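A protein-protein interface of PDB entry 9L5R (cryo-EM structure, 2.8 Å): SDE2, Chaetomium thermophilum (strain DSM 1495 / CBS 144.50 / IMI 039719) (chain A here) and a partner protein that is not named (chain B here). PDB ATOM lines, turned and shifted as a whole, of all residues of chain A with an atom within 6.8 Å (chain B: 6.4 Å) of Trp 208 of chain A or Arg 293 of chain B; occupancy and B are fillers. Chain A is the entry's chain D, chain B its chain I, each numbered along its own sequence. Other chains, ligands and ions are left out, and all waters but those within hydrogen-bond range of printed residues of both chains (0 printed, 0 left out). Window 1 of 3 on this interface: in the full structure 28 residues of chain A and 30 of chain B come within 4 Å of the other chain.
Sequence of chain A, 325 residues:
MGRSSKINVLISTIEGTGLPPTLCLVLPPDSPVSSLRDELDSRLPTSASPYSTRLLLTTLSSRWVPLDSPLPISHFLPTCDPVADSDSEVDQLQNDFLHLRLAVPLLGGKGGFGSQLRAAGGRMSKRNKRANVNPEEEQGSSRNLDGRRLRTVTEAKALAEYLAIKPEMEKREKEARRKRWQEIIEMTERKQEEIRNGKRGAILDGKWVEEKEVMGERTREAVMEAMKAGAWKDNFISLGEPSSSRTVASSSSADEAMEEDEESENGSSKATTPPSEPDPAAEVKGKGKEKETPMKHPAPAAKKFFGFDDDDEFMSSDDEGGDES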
ATOM      1  N   ASP A 205      31.684  16.792 -21.758  1.00  0.00           N
ATOM      2  CA  ASP A 205      31.518  18.213 -21.472  1.00  0.00           C
ATOM      3  C   ASP A 205      30.161  18.481 -20.829  1.00  0.00           C
ATOM      4  O   ASP A 205      29.454  17.546 -20.456  1.00  0.00           O
ATOM      5  CB  ASP A 205      31.681  19.036 -22.749  1.00  0.00           C
ATOM      6  CG  ASP A 205      33.134  19.200 -23.154  1.00  0.00           C
ATOM      7  OD1 ASP A 205      34.019  18.975 -22.302  1.00  0.00           O
ATOM      8  OD2 ASP A 205      33.391  19.552 -24.325  1.00  0.00           O
ATOM      9  N   GLY A 206      29.806  19.762 -20.698  1.00  0.00           N
ATOM     10  CA  GLY A 206      28.570  20.114 -20.015  1.00  0.00           C
ATOM     11  C   GLY A 206      27.327  19.723 -20.793  1.00  0.00           C
ATOM     12  O   GLY A 206      26.398  19.119 -20.243  1.00  0.00           O
ATOM     13  N   LYS A 207      27.287  20.068 -22.085  1.00  0.00           N
ATOM     14  CA  LYS A 207      26.160  19.653 -22.912  1.00  0.00           C
ATOM     15  C   LYS A 207      26.078  18.134 -22.973  1.00  0.00           C
ATOM     16  O   LYS A 207      24.983  17.565 -22.936  1.00  0.00           O
ATOM     17  CB  LYS A 207      26.257  20.292 -24.306  1.00  0.00           C
ATOM     18  CG  LYS A 207      27.450  19.903 -25.201  1.00  0.00           C
ATOM     19  CD  LYS A 207      27.165  18.696 -26.101  1.00  0.00           C
ATOM     20  CE  LYS A 207      28.323  18.412 -27.040  1.00  0.00           C
ATOM     21  NZ  LYS A 207      28.056  17.225 -27.900  1.00  0.00           N
ATOM     22  N   TRP A 208      27.239  17.471 -22.960  1.00  0.00           N
ATOM     23  CA  TRP A 208      27.302  16.015 -22.912  1.00  0.00           C
ATOM     24  C   TRP A 208      26.623  15.473 -21.656  1.00  0.00           C
ATOM     25  O   TRP A 208      25.721  14.632 -21.742  1.00  0.00           O
ATOM     26  CB  TRP A 208      28.768  15.577 -22.957  1.00  0.00           C
ATOM     27  CG  TRP A 208      29.008  14.161 -23.361  1.00  0.00           C
ATOM     28  CD1 TRP A 208      28.550  13.541 -24.482  1.00  0.00           C
ATOM     29  CD2 TRP A 208      29.745  13.174 -22.628  1.00  0.00           C
ATOM     30  NE1 TRP A 208      28.972  12.233 -24.508  1.00  0.00           N
ATOM     31  CE2 TRP A 208      29.703  11.982 -23.376  1.00  0.00           C
ATOM     32  CE3 TRP A 208      30.440  13.187 -21.415  1.00  0.00           C
ATOM     33  CZ2 TRP A 208      30.329  10.812 -22.951  1.00  0.00           C
ATOM     34  CZ3 TRP A 208      31.062  12.025 -20.995  1.00  0.00           C
ATOM     35  CH2 TRP A 208      31.003  10.854 -21.761  1.00  0.00           C
ATOM     36  N   VAL A 209      27.011  15.982 -20.481  1.00  0.00           N
ATOM     37  CA  VAL A 209      26.575  15.361 -19.231  1.00  0.00           C
ATOM     38  C   VAL A 209      25.105  15.673 -18.937  1.00  0.00           C
ATOM     39  O   VAL A 209      24.354  14.790 -18.499  1.00  0.00           O
ATOM     40  CB  VAL A 209      27.515  15.745 -18.066  1.00  0.00           C
ATOM     41  CG1 VAL A 209      27.575  17.246 -17.827  1.00  0.00           C
ATOM     42  CG2 VAL A 209      27.126  15.008 -16.787  1.00  0.00           C
ATOM     43  N   GLU A 210      24.646  16.907 -19.193  1.00  0.00           N
ATOM     44  CA  GLU A 210      23.205  17.128 -19.041  1.00  0.00           C
ATOM     45  C   GLU A 210      22.374  16.502 -20.160  1.00  0.00           C
ATOM     46  O   GLU A 210      21.203  16.187 -19.925  1.00  0.00           O
ATOM     47  CB  GLU A 210      22.843  18.608 -18.837  1.00  0.00           C
ATOM     48  CG  GLU A 210      23.046  19.152 -17.392  1.00  0.00           C
ATOM     49  CD  GLU A 210      24.432  19.618 -17.004  1.00  0.00           C
ATOM     50  OE1 GLU A 210      25.335  19.633 -17.842  1.00  0.00           O
ATOM     51  OE2 GLU A 210      24.615  19.975 -15.820  1.00  0.00           O
ATOM     52  N   GLU A 211      22.942  16.241 -21.346  1.00  0.00           N
ATOM     53  CA  GLU A 211      22.212  15.421 -22.310  1.00  0.00           C
ATOM     54  C   GLU A 211      22.056  13.989 -21.809  1.00  0.00           C
ATOM     55  O   GLU A 211      20.995  13.373 -21.985  1.00  0.00           O
ATOM     56  CB  GLU A 211      22.906  15.444 -23.672  1.00  0.00           C
ATOM     57  CG  GLU A 211      22.411  16.547 -24.594  1.00  0.00           C
ATOM     58  CD  GLU A 211      23.100  16.533 -25.943  1.00  0.00           C
ATOM     59  OE1 GLU A 211      24.031  15.723 -26.130  1.00  0.00           O
ATOM     60  OE2 GLU A 211      22.707  17.333 -26.818  1.00  0.00           O
ATOM     61  N   LYS A 212      23.095  13.454 -21.164  1.00  0.00           N
ATOM     62  CA  LYS A 212      23.000  12.108 -20.603  1.00  0.00           C
ATOM     63  C   LYS A 212      21.967  12.055 -19.483  1.00  0.00           C
ATOM     64  O   LYS A 212      21.150  11.126 -19.420  1.00  0.00           O
ATOM     65  CB  LYS A 212      24.368  11.640 -20.090  1.00  0.00           C
ATOM     66  CG  LYS A 212      25.482  11.548 -21.142  1.00  0.00           C
ATOM     67  CD  LYS A 212      24.947  11.187 -22.514  1.00  0.00           C
ATOM     68  CE  LYS A 212      25.792  11.718 -23.640  1.00  0.00           C
ATOM     69  NZ  LYS A 212      25.053  11.688 -24.932  1.00  0.00           N
ATOM     70  N   GLU A 213      21.971  13.066 -18.610  1.00  0.00           N
ATOM     71  CA  GLU A 213      21.007  13.110 -17.513  1.00  0.00           C
ATOM     72  C   GLU A 213      19.578  13.264 -18.026  1.00  0.00           C
ATOM     73  O   GLU A 213      18.651  12.617 -17.511  1.00  0.00           O
ATOM     74  CB  GLU A 213      21.365  14.246 -16.555  1.00  0.00           C
ATOM     75  CG  GLU A 213      20.888  14.035 -15.128  1.00  0.00           C
ATOM     76  CD  GLU A 213      21.276  15.178 -14.211  1.00  0.00           C
ATOM     77  OE1 GLU A 213      22.479  15.316 -13.905  1.00  0.00           O
ATOM     78  OE2 GLU A 213      20.378  15.939 -13.794  1.00  0.00           O
ATOM     79  N   ASP B 256      28.470  12.494 -35.454  1.00  0.00           N
ATOM     80  CA  ASP B 256      28.845  13.030 -34.148  1.00  0.00           C
ATOM     81  C   ASP B 256      27.866  12.595 -33.064  1.00  0.00           C
ATOM     82  O   ASP B 256      28.275  12.291 -31.937  1.00  0.00           O
ATOM     83  CB  ASP B 256      28.932  14.555 -34.216  1.00  0.00           C
ATOM     84  CG  ASP B 256      27.704  15.184 -34.851  1.00  0.00           C
ATOM     85  OD1 ASP B 256      26.848  14.436 -35.369  1.00  0.00           O
ATOM     86  OD2 ASP B 256      27.596  16.427 -34.830  1.00  0.00           O
ATOM     87  N   GLN B 257      26.576  12.558 -33.382  1.00  0.00           N
ATOM     88  CA  GLN B 257      25.531  12.190 -32.434  1.00  0.00           C
ATOM     89  C   GLN B 257      24.901  10.851 -32.800  1.00  0.00           C
ATOM     90  O   GLN B 257      23.687  10.659 -32.680  1.00  0.00           O
ATOM     91  CB  GLN B 257      24.474  13.286 -32.350  1.00  0.00           C
ATOM     92  CG  GLN B 257      25.060  14.663 -32.100  1.00  0.00           C
ATOM     93  CD  GLN B 257      26.015  14.683 -30.923  1.00  0.00           C
ATOM     94  OE1 GLN B 257      25.662  14.280 -29.816  1.00  0.00           O
ATOM     95  NE2 GLN B 257      27.233  15.155 -31.159  1.00  0.00           N
ATOM     96  N   THR B 291      32.549   4.962 -31.363  1.00  0.00           N
ATOM     97  CA  THR B 291      32.871   6.005 -30.399  1.00  0.00           C
ATOM     98  C   THR B 291      32.648   5.466 -28.995  1.00  0.00           C
ATOM     99  O   THR B 291      31.587   4.904 -28.706  1.00  0.00           O
ATOM    100  CB  THR B 291      32.018   7.257 -30.633  1.00  0.00           C
ATOM    101  OG1 THR B 291      32.293   7.785 -31.936  1.00  0.00           O
ATOM    102  CG2 THR B 291      32.320   8.324 -29.589  1.00  0.00           C
ATOM    103  N   VAL B 292      33.657   5.628 -28.134  1.00  0.00           N
ATOM    104  CA  VAL B 292      33.547   5.175 -26.751  1.00  0.00           C
ATOM    105  C   VAL B 292      32.490   5.979 -26.005  1.00  0.00           C
ATOM    106  O   VAL B 292      31.726   5.427 -25.206  1.00  0.00           O
ATOM    107  CB  VAL B 292      34.921   5.252 -26.061  1.00  0.00           C
ATOM    108  CG1 VAL B 292      34.833   4.793 -24.616  1.00  0.00           C
ATOM    109  CG2 VAL B 292      35.916   4.401 -26.818  1.00  0.00           C
ATOM    110  N   ARG B 293      32.421   7.289 -26.266  1.00  0.00           N
ATOM    111  CA  ARG B 293      31.401   8.130 -25.642  1.00  0.00           C
ATOM    112  C   ARG B 293      29.999   7.661 -26.006  1.00  0.00           C
ATOM    113  O   ARG B 293      29.135   7.513 -25.133  1.00  0.00           O
ATOM    114  CB  ARG B 293      31.594   9.585 -26.065  1.00  0.00           C
ATOM    115  CG  ARG B 293      32.958  10.160 -25.751  1.00  0.00           C
ATOM    116  CD  ARG B 293      33.248  11.392 -26.596  1.00  0.00           C
ATOM    117  NE  ARG B 293      32.306  12.477 -26.350  1.00  0.00           N
ATOM    118  CZ  ARG B 293      31.387  12.882 -27.218  1.00  0.00           C
ATOM    119  NH1 ARG B 293      31.251  12.305 -28.400  1.00  0.00           N
ATOM    120  NH2 ARG B 293      30.587  13.893 -26.891  1.00  0.00           N
ATOM    121  N   ASP B 294      29.770   7.401 -27.297  1.00  0.00           N
ATOM    122  CA  ASP B 294      28.464   6.937 -27.753  1.00  0.00           C
ATOM    123  C   ASP B 294      28.140   5.551 -27.208  1.00  0.00           C
ATOM    124  O   ASP B 294      27.010   5.299 -26.768  1.00  0.00           O
ATOM    125  CB  ASP B 294      28.411   6.951 -29.278  1.00  0.00           C
ATOM    126  CG  ASP B 294      28.669   8.328 -29.856  1.00  0.00           C
ATOM    127  OD1 ASP B 294      28.567   9.318 -29.100  1.00  0.00           O
ATOM    128  OD2 ASP B 294      28.954   8.425 -31.067  1.00  0.00           O
ATOM    129  N   PHE B 295      29.129   4.652 -27.200  1.00  0.00           N
ATOM    130  CA  PHE B 295      28.939   3.316 -26.640  1.00  0.00           C
ATOM    131  C   PHE B 295      28.557   3.372 -25.168  1.00  0.00           C
ATOM    132  O   PHE B 295      27.664   2.643 -24.719  1.00  0.00           O
ATOM    133  CB  PHE B 295      30.213   2.490 -26.822  1.00  0.00           C
ATOM    134  CG  PHE B 295      30.152   1.133 -26.182  1.00  0.00           C
ATOM    135  CD1 PHE B 295      29.419   0.109 -26.754  1.00  0.00           C
ATOM    136  CD2 PHE B 295      30.837   0.883 -25.001  1.00  0.00           C
ATOM    137  CE1 PHE B 295      29.366  -1.138 -26.156  1.00  0.00           C
ATOM    138  CE2 PHE B 295      30.787  -0.360 -24.400  1.00  0.00           C
ATOM    139  CZ  PHE B 295      30.051  -1.371 -24.978  1.00  0.00           C
ATOM    140  N   THR B 296      29.197   4.251 -24.406  1.00  0.00           N
ATOM    141  CA  THR B 296      28.972   4.238 -22.969  1.00  0.00           C
ATOM    142  C   THR B 296      27.726   5.017 -22.567  1.00  0.00           C
ATOM    143  O   THR B 296      27.086   4.659 -21.574  1.00  0.00           O
ATOM    144  CB  THR B 296      30.213   4.758 -22.261  1.00  0.00           C
ATOM    145  OG1 THR B 296      30.598   6.015 -22.829  1.00  0.00           O
ATOM    146  CG2 THR B 296      31.326   3.759 -22.486  1.00  0.00           C
ATOM    147  N   MET B 297      27.331   6.045 -23.327  1.00  0.00           N
ATOM    148  CA  MET B 297      26.016   6.633 -23.083  1.00  0.00           C
ATOM    149  C   MET B 297      24.905   5.665 -23.477  1.00  0.00           C
ATOM    150  O   MET B 297      23.856   5.613 -22.820  1.00  0.00           O
ATOM    151  CB  MET B 297      25.881   7.980 -23.804  1.00  0.00           C
ATOM    152  CG  MET B 297      26.006   7.969 -25.317  1.00  0.00           C
ATOM    153  SD  MET B 297      24.598   7.456 -26.314  1.00  0.00           S
ATOM    154  CE  MET B 297      23.500   8.842 -26.085  1.00  0.00           C
ATOM    155  N   ILE B 298      25.137   4.863 -24.524  1.00  0.00           N
ATOM    156  CA  ILE B 298      24.206   3.796 -24.878  1.00  0.00           C
ATOM    157  C   ILE B 298      24.095   2.783 -23.742  1.00  0.00           C
ATOM    158  O   ILE B 298      22.991   2.385 -23.354  1.00  0.00           O
ATOM    159  CB  ILE B 298      24.647   3.145 -26.206  1.00  0.00           C
ATOM    160  CG1 ILE B 298      24.127   3.955 -27.396  1.00  0.00           C
ATOM    161  CG2 ILE B 298      24.192   1.707 -26.312  1.00  0.00           C
ATOM    162  CD1 ILE B 298      24.745   3.550 -28.713  1.00  0.00           C
ATOM    163  N   VAL B 355      35.307  -1.381 -29.315  1.00  0.00           N
ATOM    164  CA  VAL B 355      35.043  -0.015 -29.761  1.00  0.00           C
ATOM    165  C   VAL B 355      36.328   0.807 -29.755  1.00  0.00           C
ATOM    166  O   VAL B 355      36.578   1.601 -30.670  1.00  0.00           O
ATOM    167  CB  VAL B 355      33.941   0.616 -28.885  1.00  0.00           C
ATOM    168  CG1 VAL B 355      33.881   2.126 -29.062  1.00  0.00           C
ATOM    169  CG2 VAL B 355      32.593   0.000 -29.217  1.00  0.00           C
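The guanidinium group (NH2) of Arg 293 of chain B lies close to the indole nitrogen (NE1) of Trp 208 of chain A.
The side-chain hydroxyl (OG1) of Thr 296 of chain B lies within hydrogen-bond range of the backbone carbonyl oxygen (O) of Arg 293 of chain B, at 3.1 Å.
Among the printed residues, pairs that only touch across the chains: Lys 212 of chain A with Met 297 of chain B and Lys 207 of chain A with Gln 257 of chain B.
Printed residues of chain A within 4 Å of Arg 293 of chain B: Trp 208. Of the printed residues of chain A, Met 297 of chain B touches Lys 212 (3.4 Å). Of the printed residues of chain A, Gln 257 of chain B touches Lys 207. Of the printed residues of chain B, Lys 212 of chain A touches Met 297 (3.4 Å). Printed residues of chain B within 4 Å of Lys 207 of chain A: Gln 257. Val 292 of chain B touches none of the printed residues of chain A. Val 355 of chain B touches none of the printed residues of chain A. The nearest printed residue of chain A that does not touch Met 297 of chain B is Trp 208 of chain A (5.3 Å).
Of the 11 printed residues of chain B, 3 touch a printed residue of chain A. Of the 9 printed residues of chain A, 3 touch a printed residue of chain B. Printed residues of chain A that touch a printed residue of chain B: Lys 207, Trp 208 and Lys 212. Hydrophobic or aromatic side chains of chain A that line the printed part of chain B: Trp 208. Among the printed residues, 3 pairs touch across the chains. Among the printed residues, no Asp or Glu carboxylate lies within 4 Å of a Lys or Arg side-chain nitrogen of the other chain.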
